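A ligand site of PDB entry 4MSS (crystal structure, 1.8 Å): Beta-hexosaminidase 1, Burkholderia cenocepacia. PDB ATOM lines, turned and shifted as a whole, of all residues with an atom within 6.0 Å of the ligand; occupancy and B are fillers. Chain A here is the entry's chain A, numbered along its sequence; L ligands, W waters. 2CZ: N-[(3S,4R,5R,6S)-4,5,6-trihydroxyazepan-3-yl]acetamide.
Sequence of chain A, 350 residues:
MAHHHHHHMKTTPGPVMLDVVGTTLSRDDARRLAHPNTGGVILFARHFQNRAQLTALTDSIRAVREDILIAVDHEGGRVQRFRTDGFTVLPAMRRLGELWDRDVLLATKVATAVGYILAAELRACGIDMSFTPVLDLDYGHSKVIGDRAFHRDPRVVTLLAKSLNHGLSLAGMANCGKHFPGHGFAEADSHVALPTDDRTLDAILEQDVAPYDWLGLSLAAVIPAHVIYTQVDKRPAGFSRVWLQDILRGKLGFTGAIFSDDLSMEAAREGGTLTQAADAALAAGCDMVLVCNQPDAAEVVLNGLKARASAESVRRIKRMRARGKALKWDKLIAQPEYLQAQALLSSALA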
ATOM      1  N   ILE A  42       4.992  18.637 -23.293  1.00  0.00           N
ATOM      2  CA  ILE A  42       4.147  19.733 -22.875  1.00  0.00           C
ATOM      3  C   ILE A  42       4.714  20.292 -21.556  1.00  0.00           C
ATOM      4  O   ILE A  42       5.091  19.544 -20.686  1.00  0.00           O
ATOM      5  CB  ILE A  42       2.672  19.295 -22.715  1.00  0.00           C
ATOM      6  CG1 ILE A  42       1.806  20.468 -22.197  1.00  0.00           C
ATOM      7  CG2 ILE A  42       2.570  18.079 -21.824  1.00  0.00           C
ATOM      8  CD1 ILE A  42       0.318  20.229 -22.311  1.00  0.00           C
ATOM      9  N   PHE A  44       4.416  22.971 -18.151  1.00  0.00           N
ATOM     10  CA  PHE A  44       3.442  23.492 -17.190  1.00  0.00           C
ATOM     11  C   PHE A  44       4.164  24.528 -16.324  1.00  0.00           C
ATOM     12  O   PHE A  44       5.355  24.725 -16.486  1.00  0.00           O
ATOM     13  CB  PHE A  44       2.874  22.363 -16.310  1.00  0.00           C
ATOM     14  CG  PHE A  44       1.954  21.431 -17.057  1.00  0.00           C
ATOM     15  CD1 PHE A  44       0.658  21.798 -17.341  1.00  0.00           C
ATOM     16  CD2 PHE A  44       2.416  20.216 -17.518  1.00  0.00           C
ATOM     17  CE1 PHE A  44      -0.187  20.947 -18.067  1.00  0.00           C
ATOM     18  CE2 PHE A  44       1.584  19.358 -18.224  1.00  0.00           C
ATOM     19  CZ  PHE A  44       0.285  19.737 -18.503  1.00  0.00           C
ATOM     20  N   ASP A  73       0.210  25.200 -22.772  1.00  0.00           N
ATOM     21  CA  ASP A  73      -1.112  25.800 -22.764  1.00  0.00           C
ATOM     22  C   ASP A  73      -0.985  27.302 -22.474  1.00  0.00           C
ATOM     23  O   ASP A  73      -0.942  27.726 -21.318  1.00  0.00           O
ATOM     24  CB  ASP A  73      -1.968  25.153 -21.699  1.00  0.00           C
ATOM     25  CG  ASP A  73      -2.193  23.686 -21.926  1.00  0.00           C
ATOM     26  OD1 ASP A  73      -2.528  23.303 -23.067  1.00  0.00           O
ATOM     27  OD2 ASP A  73      -2.074  22.920 -20.931  1.00  0.00           O
ATOM     28  N   GLU A  75      -3.282  30.184 -23.392  1.00  0.00           N
ATOM     29  CA  GLU A  75      -4.547  30.698 -23.927  1.00  0.00           C
ATOM     30  C   GLU A  75      -4.692  32.156 -23.548  1.00  0.00           C
ATOM     31  O   GLU A  75      -5.192  32.948 -24.331  1.00  0.00           O
ATOM     32  CB  GLU A  75      -5.746  29.913 -23.362  1.00  0.00           C
ATOM     33  CG  GLU A  75      -5.714  28.404 -23.597  1.00  0.00           C
ATOM     34  CD  GLU A  75      -6.875  27.677 -22.936  1.00  0.00           C
ATOM     35  OE1 GLU A  75      -7.880  28.352 -22.613  1.00  0.00           O
ATOM     36  OE2 GLU A  75      -6.750  26.427 -22.769  1.00  0.00           O
ATOM     37  N   ARG A  81       0.600  29.345 -18.516  1.00  0.00           N
ATOM     38  CA  ARG A  81       1.574  28.737 -17.609  1.00  0.00           C
ATOM     39  C   ARG A  81       2.693  29.714 -17.210  1.00  0.00           C
ATOM     40  O   ARG A  81       3.106  29.678 -16.066  1.00  0.00           O
ATOM     41  CB  ARG A  81       2.196  27.484 -18.228  1.00  0.00           C
ATOM     42  CG  ARG A  81       1.187  26.462 -18.715  1.00  0.00           C
ATOM     43  CD  ARG A  81       0.186  26.047 -17.644  1.00  0.00           C
ATOM     44  NE  ARG A  81      -0.798  25.108 -18.168  1.00  0.00           N
ATOM     45  CZ  ARG A  81      -2.009  24.896 -17.629  1.00  0.00           C
ATOM     46  NH1 ARG A  81      -2.396  25.567 -16.550  1.00  0.00           N
ATOM     47  NH2 ARG A  81      -2.816  24.023 -18.185  1.00  0.00           N
ATOM     48  N   PHE A 131      -1.343  25.334 -27.221  1.00  0.00           N
ATOM     49  CA  PHE A 131      -2.624  24.682 -27.440  1.00  0.00           C
ATOM     50  C   PHE A 131      -3.742  25.723 -27.313  1.00  0.00           C
ATOM     51  O   PHE A 131      -4.430  25.834 -26.295  1.00  0.00           O
ATOM     52  CB  PHE A 131      -2.805  23.505 -26.472  1.00  0.00           C
ATOM     53  CG  PHE A 131      -1.947  22.310 -26.802  1.00  0.00           C
ATOM     54  CD1 PHE A 131      -2.074  21.666 -28.023  1.00  0.00           C
ATOM     55  CD2 PHE A 131      -0.994  21.851 -25.905  1.00  0.00           C
ATOM     56  CE1 PHE A 131      -1.286  20.555 -28.320  1.00  0.00           C
ATOM     57  CE2 PHE A 131      -0.214  20.742 -26.192  1.00  0.00           C
ATOM     58  CZ  PHE A 131      -0.336  20.106 -27.409  1.00  0.00           C
ATOM     59  N   VAL A 144     -15.647  24.671 -16.630  1.00  0.00           N
ATOM     60  CA  VAL A 144     -14.257  24.375 -17.000  1.00  0.00           C
ATOM     61  C   VAL A 144     -13.788  25.237 -18.176  1.00  0.00           C
ATOM     62  O   VAL A 144     -12.654  25.677 -18.199  1.00  0.00           O
ATOM     63  CB  VAL A 144     -14.005  22.878 -17.288  1.00  0.00           C
ATOM     64  CG1 VAL A 144     -14.814  22.380 -18.445  1.00  0.00           C
ATOM     65  CG2 VAL A 144     -12.514  22.610 -17.527  1.00  0.00           C
ATOM     66  N   ILE A 145     -14.682  25.490 -19.152  1.00  0.00           N
ATOM     67  CA  ILE A 145     -14.402  26.432 -20.208  1.00  0.00           C
ATOM     68  C   ILE A 145     -14.574  27.869 -19.720  1.00  0.00           C
ATOM     69  O   ILE A 145     -13.588  28.645 -19.689  1.00  0.00           O
ATOM     70  CB  ILE A 145     -15.247  26.172 -21.490  1.00  0.00           C
ATOM     71  CG1 ILE A 145     -15.116  24.714 -21.925  1.00  0.00           C
ATOM     72  CG2 ILE A 145     -14.836  27.111 -22.614  1.00  0.00           C
ATOM     73  CD1 ILE A 145     -13.695  24.200 -22.095  1.00  0.00           C
ATOM     74  N   ARG A 148     -12.684  31.105 -21.035  1.00  0.00           N
ATOM     75  CA  ARG A 148     -11.733  30.676 -22.055  1.00  0.00           C
ATOM     76  C   ARG A 148     -12.358  30.707 -23.439  1.00  0.00           C
ATOM     77  O   ARG A 148     -11.631  30.630 -24.449  1.00  0.00           O
ATOM     78  CB  ARG A 148     -11.216  29.264 -21.752  1.00  0.00           C
ATOM     79  CG  ARG A 148     -10.403  29.148 -20.479  1.00  0.00           C
ATOM     80  CD  ARG A 148     -10.387  27.731 -20.011  1.00  0.00           C
ATOM     81  NE  ARG A 148      -9.592  26.877 -20.886  1.00  0.00           N
ATOM     82  CZ  ARG A 148      -9.613  25.561 -20.817  1.00  0.00           C
ATOM     83  NH1 ARG A 148     -10.451  24.960 -19.972  1.00  0.00           N
ATOM     84  NH2 ARG A 148      -8.825  24.832 -21.623  1.00  0.00           N
ATOM     85  N   LYS A 178      -9.805  23.681 -29.964  1.00  0.00           N
ATOM     86  CA  LYS A 178     -10.246  22.708 -28.969  1.00  0.00           C
ATOM     87  C   LYS A 178     -11.522  23.202 -28.300  1.00  0.00           C
ATOM     88  O   LYS A 178     -11.815  24.409 -28.357  1.00  0.00           O
ATOM     89  CB  LYS A 178      -9.134  22.500 -27.944  1.00  0.00           C
ATOM     90  CG  LYS A 178      -8.809  23.696 -27.071  1.00  0.00           C
ATOM     91  CD  LYS A 178      -7.514  23.517 -26.260  1.00  0.00           C
ATOM     92  CE  LYS A 178      -7.347  24.625 -25.210  1.00  0.00           C
ATOM     93  NZ  LYS A 178      -6.051  24.544 -24.475  1.00  0.00           N
ATOM     94  N   HIS A 179     -12.311  22.324 -27.677  1.00  0.00           N
ATOM     95  CA  HIS A 179     -12.139  20.875 -27.608  1.00  0.00           C
ATOM     96  C   HIS A 179     -13.231  20.232 -28.469  1.00  0.00           C
ATOM     97  O   HIS A 179     -14.415  20.205 -28.107  1.00  0.00           O
ATOM     98  CB  HIS A 179     -12.286  20.419 -26.141  1.00  0.00           C
ATOM     99  CG  HIS A 179     -11.403  21.181 -25.199  1.00  0.00           C
ATOM    100  ND1 HIS A 179     -11.693  22.459 -24.783  1.00  0.00           N
ATOM    101  CD2 HIS A 179     -10.202  20.879 -24.673  1.00  0.00           C
ATOM    102  CE1 HIS A 179     -10.722  22.885 -23.987  1.00  0.00           C
ATOM    103  NE2 HIS A 179      -9.791  21.957 -23.925  1.00  0.00           N
ATOM    104  N   HIS A 183     -16.869  21.542 -26.094  1.00  0.00           N
ATOM    105  CA  HIS A 183     -16.976  21.308 -24.655  1.00  0.00           C
ATOM    106  C   HIS A 183     -17.897  22.361 -24.010  1.00  0.00           C
ATOM    107  O   HIS A 183     -18.131  22.347 -22.812  1.00  0.00           O
ATOM    108  CB  HIS A 183     -15.587  21.359 -24.029  1.00  0.00           C
ATOM    109  CG  HIS A 183     -15.426  20.502 -22.797  1.00  0.00           C
ATOM    110  ND1 HIS A 183     -16.263  20.575 -21.710  1.00  0.00           N
ATOM    111  CD2 HIS A 183     -14.471  19.578 -22.488  1.00  0.00           C
ATOM    112  CE1 HIS A 183     -15.859  19.708 -20.792  1.00  0.00           C
ATOM    113  NE2 HIS A 183     -14.761  19.112 -21.225  1.00  0.00           N
ATOM    114  N   ASP A 189     -16.962  18.936 -15.714  1.00  0.00           N
ATOM    115  CA  ASP A 189     -15.554  19.201 -15.947  1.00  0.00           C
ATOM    116  C   ASP A 189     -14.855  17.886 -16.224  1.00  0.00           C
ATOM    117  O   ASP A 189     -14.795  17.013 -15.361  1.00  0.00           O
ATOM    118  CB  ASP A 189     -14.973  19.854 -14.695  1.00  0.00           C
ATOM    119  CG  ASP A 189     -13.493  20.203 -14.829  1.00  0.00           C
ATOM    120  OD1 ASP A 189     -12.861  19.869 -15.843  1.00  0.00           O
ATOM    121  OD2 ASP A 189     -12.955  20.807 -13.867  1.00  0.00           O
ATOM    122  N   SER A 190     -14.278  17.766 -17.421  1.00  0.00           N
ATOM    123  CA  SER A 190     -13.668  16.517 -17.841  1.00  0.00           C
ATOM    124  C   SER A 190     -12.387  16.175 -17.073  1.00  0.00           C
ATOM    125  O   SER A 190     -11.866  15.047 -17.180  1.00  0.00           O
ATOM    126  CB  SER A 190     -13.425  16.513 -19.367  1.00  0.00           C
ATOM    127  OG  SER A 190     -12.774  17.707 -19.780  1.00  0.00           O
ATOM    128  N   HIS A 191     -11.854  17.137 -16.301  1.00  0.00           N
ATOM    129  CA  HIS A 191     -10.685  16.824 -15.462  1.00  0.00           C
ATOM    130  C   HIS A 191     -11.052  15.856 -14.381  1.00  0.00           C
ATOM    131  O   HIS A 191     -10.234  15.065 -13.945  1.00  0.00           O
ATOM    132  CB  HIS A 191     -10.109  18.049 -14.776  1.00  0.00           C
ATOM    133  CG  HIS A 191      -9.382  18.990 -15.685  1.00  0.00           C
ATOM    134  ND1 HIS A 191     -10.014  20.038 -16.318  1.00  0.00           N
ATOM    135  CD2 HIS A 191      -8.073  19.050 -16.042  1.00  0.00           C
ATOM    136  CE1 HIS A 191      -9.126  20.703 -17.041  1.00  0.00           C
ATOM    137  NE2 HIS A 191      -7.943  20.132 -16.882  1.00  0.00           N
ATOM    138  N   ILE A 223      -7.587  19.458 -30.648  1.00  0.00           N
ATOM    139  CA  ILE A 223      -7.716  18.538 -29.502  1.00  0.00           C
ATOM    140  C   ILE A 223      -9.171  18.201 -29.350  1.00  0.00           C
ATOM    141  O   ILE A 223      -9.995  19.115 -29.289  1.00  0.00           O
ATOM    142  CB  ILE A 223      -7.252  19.176 -28.168  1.00  0.00           C
ATOM    143  CG1 ILE A 223      -5.746  19.280 -28.147  1.00  0.00           C
ATOM    144  CG2 ILE A 223      -7.705  18.348 -26.975  1.00  0.00           C
ATOM    145  CD1 ILE A 223      -5.183  20.244 -27.106  1.00  0.00           C
ATOM    146  N   ASP A 261      -6.861  15.024 -25.787  1.00  0.00           N
ATOM    147  CA  ASP A 261      -6.732  15.745 -24.531  1.00  0.00           C
ATOM    148  C   ASP A 261      -6.051  14.777 -23.570  1.00  0.00           C
ATOM    149  O   ASP A 261      -5.937  13.578 -23.855  1.00  0.00           O
ATOM    150  CB  ASP A 261      -8.096  16.216 -24.001  1.00  0.00           C
ATOM    151  CG  ASP A 261      -7.976  17.410 -23.037  1.00  0.00           C
ATOM    152  OD1 ASP A 261      -6.848  17.715 -22.581  1.00  0.00           O
ATOM    153  OD2 ASP A 261      -9.015  18.008 -22.730  1.00  0.00           O
ATOM    154  N   ASP A 262      -5.562  15.318 -22.465  1.00  0.00           N
ATOM    155  CA  ASP A 262      -4.743  14.615 -21.504  1.00  0.00           C
ATOM    156  C   ASP A 262      -5.428  13.319 -21.030  1.00  0.00           C
ATOM    157  O   ASP A 262      -6.527  13.326 -20.469  1.00  0.00           O
ATOM    158  CB  ASP A 262      -4.442  15.586 -20.328  1.00  0.00           C
ATOM    159  CG  ASP A 262      -3.667  14.935 -19.182  1.00  0.00           C
ATOM    160  OD1 ASP A 262      -3.071  13.864 -19.411  1.00  0.00           O
ATOM    161  OD2 ASP A 262      -3.656  15.498 -18.052  1.00  0.00           O
ATOM    162  N   MET A 265      -6.677  12.833 -17.299  1.00  0.00           N
ATOM    163  CA  MET A 265      -7.932  13.393 -16.841  1.00  0.00           C
ATOM    164  C   MET A 265      -8.957  12.295 -16.548  1.00  0.00           C
ATOM    165  O   MET A 265      -8.988  11.267 -17.219  1.00  0.00           O
ATOM    166  CB  MET A 265      -8.484  14.345 -17.898  1.00  0.00           C
ATOM    167  CG  MET A 265      -7.595  15.539 -18.158  1.00  0.00           C
ATOM    168  SD  MET A 265      -8.084  16.477 -19.635  1.00  0.00           S
ATOM    169  CE  MET A 265      -9.586  17.288 -19.127  1.00  0.00           C
ATOM    170  N   LEU A 290      -1.654  12.957 -25.385  1.00  0.00           N
ATOM    171  CA  LEU A 290      -1.055  13.638 -24.240  1.00  0.00           C
ATOM    172  C   LEU A 290      -1.168  12.775 -22.990  1.00  0.00           C
ATOM    173  O   LEU A 290      -2.268  12.295 -22.652  1.00  0.00           O
ATOM    174  CB  LEU A 290      -1.779  14.961 -23.994  1.00  0.00           C
ATOM    175  CG  LEU A 290      -1.242  16.187 -24.767  1.00  0.00           C
ATOM    176  CD1 LEU A 290      -1.148  15.958 -26.297  1.00  0.00           C
ATOM    177  CD2 LEU A 290      -2.097  17.398 -24.473  1.00  0.00           C
ATOM    178  N   CYS A 292      -0.136  13.698 -19.205  1.00  0.00           N
ATOM    179  CA  CYS A 292       0.425  14.749 -18.379  1.00  0.00           C
ATOM    180  C   CYS A 292       0.536  14.376 -16.918  1.00  0.00           C
ATOM    181  O   CYS A 292      -0.300  13.654 -16.382  1.00  0.00           O
ATOM    182  CB  CYS A 292      -0.420  16.023 -18.486  1.00  0.00           C
ATOM    183  SG  CYS A 292      -0.709  16.521 -20.223  1.00  0.00           S
HETATM  184  N1  2CZ L   1      -5.792  18.984 -20.610  1.00  0.00           N
HETATM  185  C2  2CZ L   1      -6.370  20.162 -19.999  1.00  0.00           C
HETATM  186  N2  2CZ L   1      -8.473  20.458 -21.134  1.00  0.00           N
HETATM  187  C3  2CZ L   1      -7.172  21.044 -20.899  1.00  0.00           C
HETATM  188  C4  2CZ L   1      -6.550  21.226 -22.285  1.00  0.00           C
HETATM  189  O4  2CZ L   1      -7.186  22.297 -22.952  1.00  0.00           O
HETATM  190  C5  2CZ L   1      -5.095  21.606 -22.252  1.00  0.00           C
HETATM  191  O5  2CZ L   1      -4.832  22.069 -23.573  1.00  0.00           O
HETATM  192  C6  2CZ L   1      -4.091  20.533 -21.819  1.00  0.00           C
HETATM  193  O6  2CZ L   1      -3.490  20.916 -20.567  1.00  0.00           O
HETATM  194  C7  2CZ L   1      -4.613  19.161 -21.487  1.00  0.00           C
HETATM  195  C8  2CZ L   1      -9.688  21.153 -20.809  1.00  0.00           C
HETATM  196  O8  2CZ L   1      -9.647  22.235 -20.256  1.00  0.00           O
HETATM  197  C9  2CZ L   1     -11.022  20.491 -21.115  1.00  0.00           C
HETATM  198  O   HOH W   1      -4.857  17.885 -18.099  1.00  0.00           O
HETATM  199  O   HOH W   2      -3.386  20.403 -17.683  1.00  0.00           O
HETATM  200  O   HOH W   3      -7.799  23.452 -18.219  1.00  0.00           O
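Residues that only touch the ligand: Arg 81, Phe 131, Val 144, His 183, Ser 190, His 191, Ile 223 and Asp 262.
Hydrophobic or aromatic side chains within 4 Å of the ligand: Phe 131, Val 144, His 179, His 183, His 191, Ile 223 and Met 265.
Of the 21 residues printed, 14 come within 4 Å of the ligand.
O6 of the ligand sits at hydrogen-bond distance from OD2 of Asp 73, at 2.5 Å.
OD1 of Asp 261 lies within salt-bridge range of N1 of the ligand.
A ring nitrogen (NE2) of His 179 lies within hydrogen-bond range of an oxygen (O4) of the ligand (2.8 Å).
The guanidinium group (NH1) of Arg 148 lies within hydrogen-bond range of an oxygen (O8) of the ligand.
NZ of Lys 178 is in hydrogen-bond range of O5 of the ligand (2.9 Å).
The side-chain sulfur of Met 265 is in hydrogen-bond range of a nitrogen (N1) of the ligand, at 3.5 Å.
Water W1 lies within hydrogen-bond range of OD2 of Asp 262 and N1 of the ligand.
The side-chain carboxylate of Asp 73 is in salt-bridge range of the side-chain amino group of Lys 178 (3.99 Å).
The side-chain carboxylate of Asp 73 lies within salt-bridge range of the guanidinium group of Arg 81 (3.1 Å).
The backbone carbonyl oxygen of Val 144 lies within hydrogen-bond range of the guanidinium group of Arg 148 (2.9 Å).
OE1 of Glu 75 lies within salt-bridge range of NE of Arg 148 (2.8 Å).
The side-chain carboxylate of Glu 75 is in salt-bridge range of the side-chain amino group of Lys 178 (2.6 Å).
The side-chain carboxylate of Asp 189 lies within hydrogen-bond range of a ring nitrogen (ND1) of His 191, 2.9 Å away.
The side-chain hydroxyl of Ser 190 is in hydrogen-bond range of a ring nitrogen (NE2) of His 183 (2.8 Å).
N of Cys 292 sits at hydrogen-bond distance from OD1 of Asp 262 (2.9 Å).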
